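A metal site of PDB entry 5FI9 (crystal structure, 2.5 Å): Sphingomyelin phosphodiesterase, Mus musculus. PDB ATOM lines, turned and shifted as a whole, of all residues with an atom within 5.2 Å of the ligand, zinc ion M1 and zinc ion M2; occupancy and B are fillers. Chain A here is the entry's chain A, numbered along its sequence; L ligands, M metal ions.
O of His 382 lies within hydrogen-bond range of N1 of the ligand (3.1 Å).
NE2 of His 244 is in hydrogen-bond range of O1 of the ligand, 2.9 Å away.
NE2 of His 207 is in hydrogen-bond range of O1 of the ligand, at 3.0 Å.
The side-chain carboxylate of Asp 131 lies within hydrogen-bond range of the backbone NH of His 382 (3.1 Å).
ND1 of His 384 is in hydrogen-bond range of O of Phe 413.
The side-chain carboxylate (OD2) of Asp 203 sits at hydrogen-bond distance from the backbone NH (N) of His 244 (3.1 Å).
The side-chain hydroxyl of Thr 383 sits at hydrogen-bond distance from the backbone carbonyl oxygen of Val 385 (3.3 Å).
O of Thr 383 touches C5 of the ligand, 3.6 Å away.
N of Ile 414 touches C6 of the ligand, at 3.8 Å.
His 500 touches the ligand (ND1 to C10, 3.5 Å).
Hydrophobic or aromatic side chains within 4 Å of the ligand: His 133, His 207, His 244, His 382, His 384 and His 500.
Of the 16 residues printed, 12 come within 4 Å of the ligand.
The nearest printed residue that does not touch the ligand is Val 385 (4.01 Å).
Within 4 Å of zinc ion M1: Asp 131, His 133, Asp 203 and His 384.
Of the 16 residues printed, 4 come within 4 Å of zinc ion M2.
Zinc ion M1 is bound by NE2 of His 133 (2.0 Å), OD1 of Asp 131 (2.0 Å), NE2 of His 384 (2.1 Å), OD1 of Asp 203 (2.3 Å) and O3 of the ligand (2.3 Å).
Zinc ion M1 has five donor atoms within binding distance.
Slightly farther from zinc ion M1 lies an oxygen (O1) of the ligand (2.7 Å).
Zinc ion M2 is bound by NE2 of His 350 (2.0 Å), OD1 of Asn 243 (2.1 Å), ND1 of His 382 (2.1 Å), OD1 of Asp 203 (2.2 Å), O2 of the ligand (2.2 Å) and O3 of the ligand (2.5 Å).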
ATOM      1  N   ASP A 131      -7.849  21.221  21.200  1.00  0.00           N
ATOM      2  CA  ASP A 131      -8.788  20.553  20.302  1.00  0.00           C
ATOM      3  C   ASP A 131      -9.680  21.558  19.588  1.00  0.00           C
ATOM      4  O   ASP A 131     -10.907  21.476  19.614  1.00  0.00           O
ATOM      5  CB  ASP A 131      -9.629  19.529  21.080  1.00  0.00           C
ATOM      6  CG  ASP A 131      -8.774  18.512  21.821  1.00  0.00           C
ATOM      7  OD1 ASP A 131      -8.486  17.446  21.249  1.00  0.00           O
ATOM      8  OD2 ASP A 131      -8.385  18.799  22.981  1.00  0.00           O
ATOM      9  N   HIS A 133      -9.622  21.999  16.249  1.00  0.00           N
ATOM     10  CA  HIS A 133     -10.100  21.218  15.107  1.00  0.00           C
ATOM     11  C   HIS A 133     -10.836  22.106  14.097  1.00  0.00           C
ATOM     12  O   HIS A 133     -12.052  22.025  13.918  1.00  0.00           O
ATOM     13  CB  HIS A 133     -11.007  20.072  15.582  1.00  0.00           C
ATOM     14  CG  HIS A 133     -10.286  19.015  16.369  1.00  0.00           C
ATOM     15  ND1 HIS A 133      -9.422  18.126  15.775  1.00  0.00           N
ATOM     16  CD2 HIS A 133     -10.312  18.700  17.679  1.00  0.00           C
ATOM     17  CE1 HIS A 133      -8.942  17.305  16.699  1.00  0.00           C
ATOM     18  NE2 HIS A 133      -9.468  17.630  17.866  1.00  0.00           N
ATOM     19  N   ASP A 203      -4.006  19.519  18.387  1.00  0.00           N
ATOM     20  CA  ASP A 203      -5.188  19.100  17.632  1.00  0.00           C
ATOM     21  C   ASP A 203      -5.833  20.301  16.930  1.00  0.00           C
ATOM     22  O   ASP A 203      -6.918  20.763  17.274  1.00  0.00           O
ATOM     23  CB  ASP A 203      -6.183  18.358  18.536  1.00  0.00           C
ATOM     24  CG  ASP A 203      -5.982  16.859  18.528  1.00  0.00           C
ATOM     25  OD1 ASP A 203      -6.862  16.126  19.037  1.00  0.00           O
ATOM     26  OD2 ASP A 203      -4.938  16.401  18.001  1.00  0.00           O
ATOM     27  N   HIS A 207     -10.935  16.429  11.449  1.00  0.00           N
ATOM     28  CA  HIS A 207     -10.848  14.979  11.341  1.00  0.00           C
ATOM     29  C   HIS A 207     -11.024  14.482   9.913  1.00  0.00           C
ATOM     30  O   HIS A 207     -11.396  13.314   9.718  1.00  0.00           O
ATOM     31  CB  HIS A 207     -11.881  14.325  12.259  1.00  0.00           C
ATOM     32  CG  HIS A 207     -11.755  14.738  13.694  1.00  0.00           C
ATOM     33  ND1 HIS A 207     -12.080  16.004  14.143  1.00  0.00           N
ATOM     34  CD2 HIS A 207     -11.357  14.047  14.790  1.00  0.00           C
ATOM     35  CE1 HIS A 207     -11.877  16.075  15.446  1.00  0.00           C
ATOM     36  NE2 HIS A 207     -11.431  14.896  15.861  1.00  0.00           N
ATOM     37  N   ASN A 243      -2.154  14.913  18.173  1.00  0.00           N
ATOM     38  CA  ASN A 243      -2.052  13.728  17.341  1.00  0.00           C
ATOM     39  C   ASN A 243      -2.615  13.910  15.941  1.00  0.00           C
ATOM     40  O   ASN A 243      -2.333  13.084  15.068  1.00  0.00           O
ATOM     41  CB  ASN A 243      -2.754  12.540  18.020  1.00  0.00           C
ATOM     42  CG  ASN A 243      -4.215  12.823  18.324  1.00  0.00           C
ATOM     43  OD1 ASN A 243      -4.561  13.871  18.855  1.00  0.00           O
ATOM     44  ND2 ASN A 243      -5.078  11.874  17.972  1.00  0.00           N
ATOM     45  N   HIS A 244      -3.380  14.973  15.698  1.00  0.00           N
ATOM     46  CA  HIS A 244      -3.910  15.259  14.364  1.00  0.00           C
ATOM     47  C   HIS A 244      -3.020  16.181  13.556  1.00  0.00           C
ATOM     48  O   HIS A 244      -3.294  16.414  12.368  1.00  0.00           O
ATOM     49  CB  HIS A 244      -5.308  15.871  14.472  1.00  0.00           C
ATOM     50  CG  HIS A 244      -6.387  14.891  14.796  1.00  0.00           C
ATOM     51  ND1 HIS A 244      -7.158  14.287  13.831  1.00  0.00           N
ATOM     52  CD2 HIS A 244      -6.826  14.407  15.983  1.00  0.00           C
ATOM     53  CE1 HIS A 244      -8.029  13.468  14.401  1.00  0.00           C
ATOM     54  NE2 HIS A 244      -7.853  13.530  15.712  1.00  0.00           N
ATOM     55  N   HIS A 350      -0.874  16.680  25.084  1.00  0.00           N
ATOM     56  CA  HIS A 350      -2.167  16.503  24.439  1.00  0.00           C
ATOM     57  C   HIS A 350      -2.887  15.278  24.994  1.00  0.00           C
ATOM     58  O   HIS A 350      -3.890  15.405  25.698  1.00  0.00           O
ATOM     59  CB  HIS A 350      -2.010  16.378  22.925  1.00  0.00           C
ATOM     60  CG  HIS A 350      -3.310  16.192  22.223  1.00  0.00           C
ATOM     61  ND1 HIS A 350      -4.297  17.156  22.216  1.00  0.00           N
ATOM     62  CD2 HIS A 350      -3.799  15.151  21.514  1.00  0.00           C
ATOM     63  CE1 HIS A 350      -5.340  16.721  21.533  1.00  0.00           C
ATOM     64  NE2 HIS A 350      -5.067  15.503  21.092  1.00  0.00           N
ATOM     65  N   HIS A 382      -7.517  16.227  24.523  1.00  0.00           N
ATOM     66  CA  HIS A 382      -7.649  15.003  23.723  1.00  0.00           C
ATOM     67  C   HIS A 382      -8.982  14.288  23.958  1.00  0.00           C
ATOM     68  O   HIS A 382      -9.534  13.693  23.024  1.00  0.00           O
ATOM     69  CB  HIS A 382      -6.484  14.055  24.023  1.00  0.00           C
ATOM     70  CG  HIS A 382      -6.410  12.880  23.096  1.00  0.00           C
ATOM     71  ND1 HIS A 382      -6.255  13.021  21.727  1.00  0.00           N
ATOM     72  CD2 HIS A 382      -6.441  11.548  23.339  1.00  0.00           C
ATOM     73  CE1 HIS A 382      -6.214  11.822  21.181  1.00  0.00           C
ATOM     74  NE2 HIS A 382      -6.326  10.912  22.130  1.00  0.00           N
ATOM     75  N   THR A 383      -9.509  14.338  25.183  1.00  0.00           N
ATOM     76  CA  THR A 383     -10.776  13.673  25.462  1.00  0.00           C
ATOM     77  C   THR A 383     -11.982  14.486  24.996  1.00  0.00           C
ATOM     78  O   THR A 383     -13.053  13.913  24.797  1.00  0.00           O
ATOM     79  CB  THR A 383     -10.915  13.410  26.965  1.00  0.00           C
ATOM     80  OG1 THR A 383     -10.915  14.649  27.681  1.00  0.00           O
ATOM     81  CG2 THR A 383      -9.774  12.540  27.459  1.00  0.00           C
ATOM     82  N   HIS A 384     -11.819  15.804  24.837  1.00  0.00           N
ATOM     83  CA  HIS A 384     -12.852  16.727  24.400  1.00  0.00           C
ATOM     84  C   HIS A 384     -13.932  16.942  25.454  1.00  0.00           C
ATOM     85  O   HIS A 384     -14.909  17.660  25.182  1.00  0.00           O
ATOM     86  CB  HIS A 384     -13.518  16.290  23.085  1.00  0.00           C
ATOM     87  CG  HIS A 384     -12.589  16.264  21.911  1.00  0.00           C
ATOM     88  ND1 HIS A 384     -13.023  16.400  20.614  1.00  0.00           N
ATOM     89  CD2 HIS A 384     -11.241  16.133  21.842  1.00  0.00           C
ATOM     90  CE1 HIS A 384     -11.992  16.344  19.788  1.00  0.00           C
ATOM     91  NE2 HIS A 384     -10.894  16.181  20.514  1.00  0.00           N
ATOM     92  N   VAL A 385     -13.801  16.365  26.647  1.00  0.00           N
ATOM     93  CA  VAL A 385     -14.765  16.524  27.724  1.00  0.00           C
ATOM     94  C   VAL A 385     -14.023  17.015  28.966  1.00  0.00           C
ATOM     95  O   VAL A 385     -12.792  16.993  29.027  1.00  0.00           O
ATOM     96  CB  VAL A 385     -15.535  15.225  28.018  1.00  0.00           C
ATOM     97  CG1 VAL A 385     -16.560  14.955  26.928  1.00  0.00           C
ATOM     98  CG2 VAL A 385     -14.580  14.046  28.151  1.00  0.00           C
ATOM     99  N   PHE A 413     -17.166  18.249  17.981  1.00  0.00           N
ATOM    100  CA  PHE A 413     -16.873  16.822  17.865  1.00  0.00           C
ATOM    101  C   PHE A 413     -16.771  16.146  19.243  1.00  0.00           C
ATOM    102  O   PHE A 413     -15.792  16.397  19.945  1.00  0.00           O
ATOM    103  CB  PHE A 413     -15.561  16.658  17.087  1.00  0.00           C
ATOM    104  CG  PHE A 413     -15.419  15.327  16.401  1.00  0.00           C
ATOM    105  CD1 PHE A 413     -15.958  15.127  15.144  1.00  0.00           C
ATOM    106  CD2 PHE A 413     -14.728  14.295  17.002  1.00  0.00           C
ATOM    107  CE1 PHE A 413     -15.818  13.909  14.505  1.00  0.00           C
ATOM    108  CE2 PHE A 413     -14.583  13.080  16.375  1.00  0.00           C
ATOM    109  CZ  PHE A 413     -15.130  12.885  15.121  1.00  0.00           C
ATOM    110  N   ILE A 414     -17.726  15.309  19.663  1.00  0.00           N
ATOM    111  CA  ILE A 414     -18.980  14.986  18.958  1.00  0.00           C
ATOM    112  C   ILE A 414     -20.156  15.341  19.852  1.00  0.00           C
ATOM    113  O   ILE A 414     -20.165  15.004  21.034  1.00  0.00           O
ATOM    114  CB  ILE A 414     -19.039  13.486  18.576  1.00  0.00           C
ATOM    115  CG1 ILE A 414     -17.920  13.128  17.603  1.00  0.00           C
ATOM    116  CG2 ILE A 414     -20.398  13.133  17.964  1.00  0.00           C
ATOM    117  CD1 ILE A 414     -17.465  11.682  17.711  1.00  0.00           C
ATOM    118  N   LEU A 416     -21.200  18.066  21.213  1.00  0.00           N
ATOM    119  CA  LEU A 416     -20.796  18.861  22.359  1.00  0.00           C
ATOM    120  C   LEU A 416     -20.925  20.339  22.022  1.00  0.00           C
ATOM    121  O   LEU A 416     -21.034  20.729  20.860  1.00  0.00           O
ATOM    122  CB  LEU A 416     -19.342  18.559  22.773  1.00  0.00           C
ATOM    123  CG  LEU A 416     -19.054  17.173  23.326  1.00  0.00           C
ATOM    124  CD1 LEU A 416     -17.551  16.901  23.319  1.00  0.00           C
ATOM    125  CD2 LEU A 416     -19.614  17.026  24.727  1.00  0.00           C
ATOM    126  N   TYR A 499     -19.449  17.552  32.351  1.00  0.00           N
ATOM    127  CA  TYR A 499     -18.634  16.640  31.562  1.00  0.00           C
ATOM    128  C   TYR A 499     -18.767  16.926  30.074  1.00  0.00           C
ATOM    129  O   TYR A 499     -17.771  17.022  29.354  1.00  0.00           O
ATOM    130  CB  TYR A 499     -19.050  15.201  31.882  1.00  0.00           C
ATOM    131  CG  TYR A 499     -18.161  14.101  31.341  1.00  0.00           C
ATOM    132  CD1 TYR A 499     -17.132  13.564  32.103  1.00  0.00           C
ATOM    133  CD2 TYR A 499     -18.377  13.575  30.074  1.00  0.00           C
ATOM    134  CE1 TYR A 499     -16.334  12.543  31.626  1.00  0.00           C
ATOM    135  CE2 TYR A 499     -17.571  12.556  29.576  1.00  0.00           C
ATOM    136  CZ  TYR A 499     -16.561  12.039  30.357  1.00  0.00           C
ATOM    137  OH  TYR A 499     -15.766  11.034  29.876  1.00  0.00           O
ATOM    138  N   HIS A 500     -20.011  17.084  29.603  1.00  0.00           N
ATOM    139  CA  HIS A 500     -20.287  17.325  28.190  1.00  0.00           C
ATOM    140  C   HIS A 500     -20.497  18.801  27.873  1.00  0.00           C
ATOM    141  O   HIS A 500     -21.145  19.131  26.881  1.00  0.00           O
ATOM    142  CB  HIS A 500     -21.513  16.519  27.760  1.00  0.00           C
ATOM    143  CG  HIS A 500     -21.439  15.065  28.105  1.00  0.00           C
ATOM    144  ND1 HIS A 500     -21.058  14.102  27.199  1.00  0.00           N
ATOM    145  CD2 HIS A 500     -21.688  14.412  29.269  1.00  0.00           C
ATOM    146  CE1 HIS A 500     -21.073  12.916  27.774  1.00  0.00           C
ATOM    147  NE2 HIS A 500     -21.450  13.075  29.038  1.00  0.00           N
HETATM  148  N1  LIG L   1      -9.648  11.540  20.825  1.00  0.00           N
HETATM  149  C1  LIG L   1      -9.995  12.106  19.569  1.00  0.00           C
HETATM  150  C2  LIG L   1     -11.426  12.588  19.578  1.00  0.00           C
HETATM  151  C3  LIG L   1     -12.243  12.022  20.711  1.00  0.00           C
HETATM  152  C4  LIG L   1     -13.718  12.283  20.518  1.00  0.00           C
HETATM  153  C5  LIG L   1     -14.454  12.366  21.839  1.00  0.00           C
HETATM  154  C6  LIG L   1     -15.941  12.566  21.652  1.00  0.00           C
HETATM  155  C7  LIG L   1     -16.635  12.919  22.946  1.00  0.00           C
HETATM  156  C8  LIG L   1     -17.615  11.851  23.366  1.00  0.00           C
HETATM  157  C9  LIG L   1     -18.391  12.250  24.602  1.00  0.00           C
HETATM  158  C10 LIG L   1     -19.780  12.726  24.251  1.00  0.00           C
HETATM  159  P1  LIG L   1      -8.885  13.487  19.176  1.00  0.00           P
HETATM  160  O1  LIG L   1      -9.455  14.286  18.034  1.00  0.00           O
HETATM  161  O2  LIG L   1      -7.536  12.949  18.772  1.00  0.00           O
HETATM  162  O3  LIG L   1      -8.747  14.367  20.394  1.00  0.00           O
HETATM  163  P2  LIG L   1      -9.814  10.842  18.272  1.00  0.00           P
HETATM  164  O4  LIG L   1      -8.574  10.025  18.541  1.00  0.00           O
HETATM  165  O5  LIG L   1      -9.697  11.528  16.924  1.00  0.00           O
HETATM  166  O6  LIG L   1     -11.029   9.946  18.270  1.00  0.00           O
HETATM  167 ZN    ZN M   1      -9.048  16.509  19.519  1.00  0.00          ZN
HETATM  168 ZN    ZN M   2      -6.278  14.268  19.994  1.00  0.00          ZN
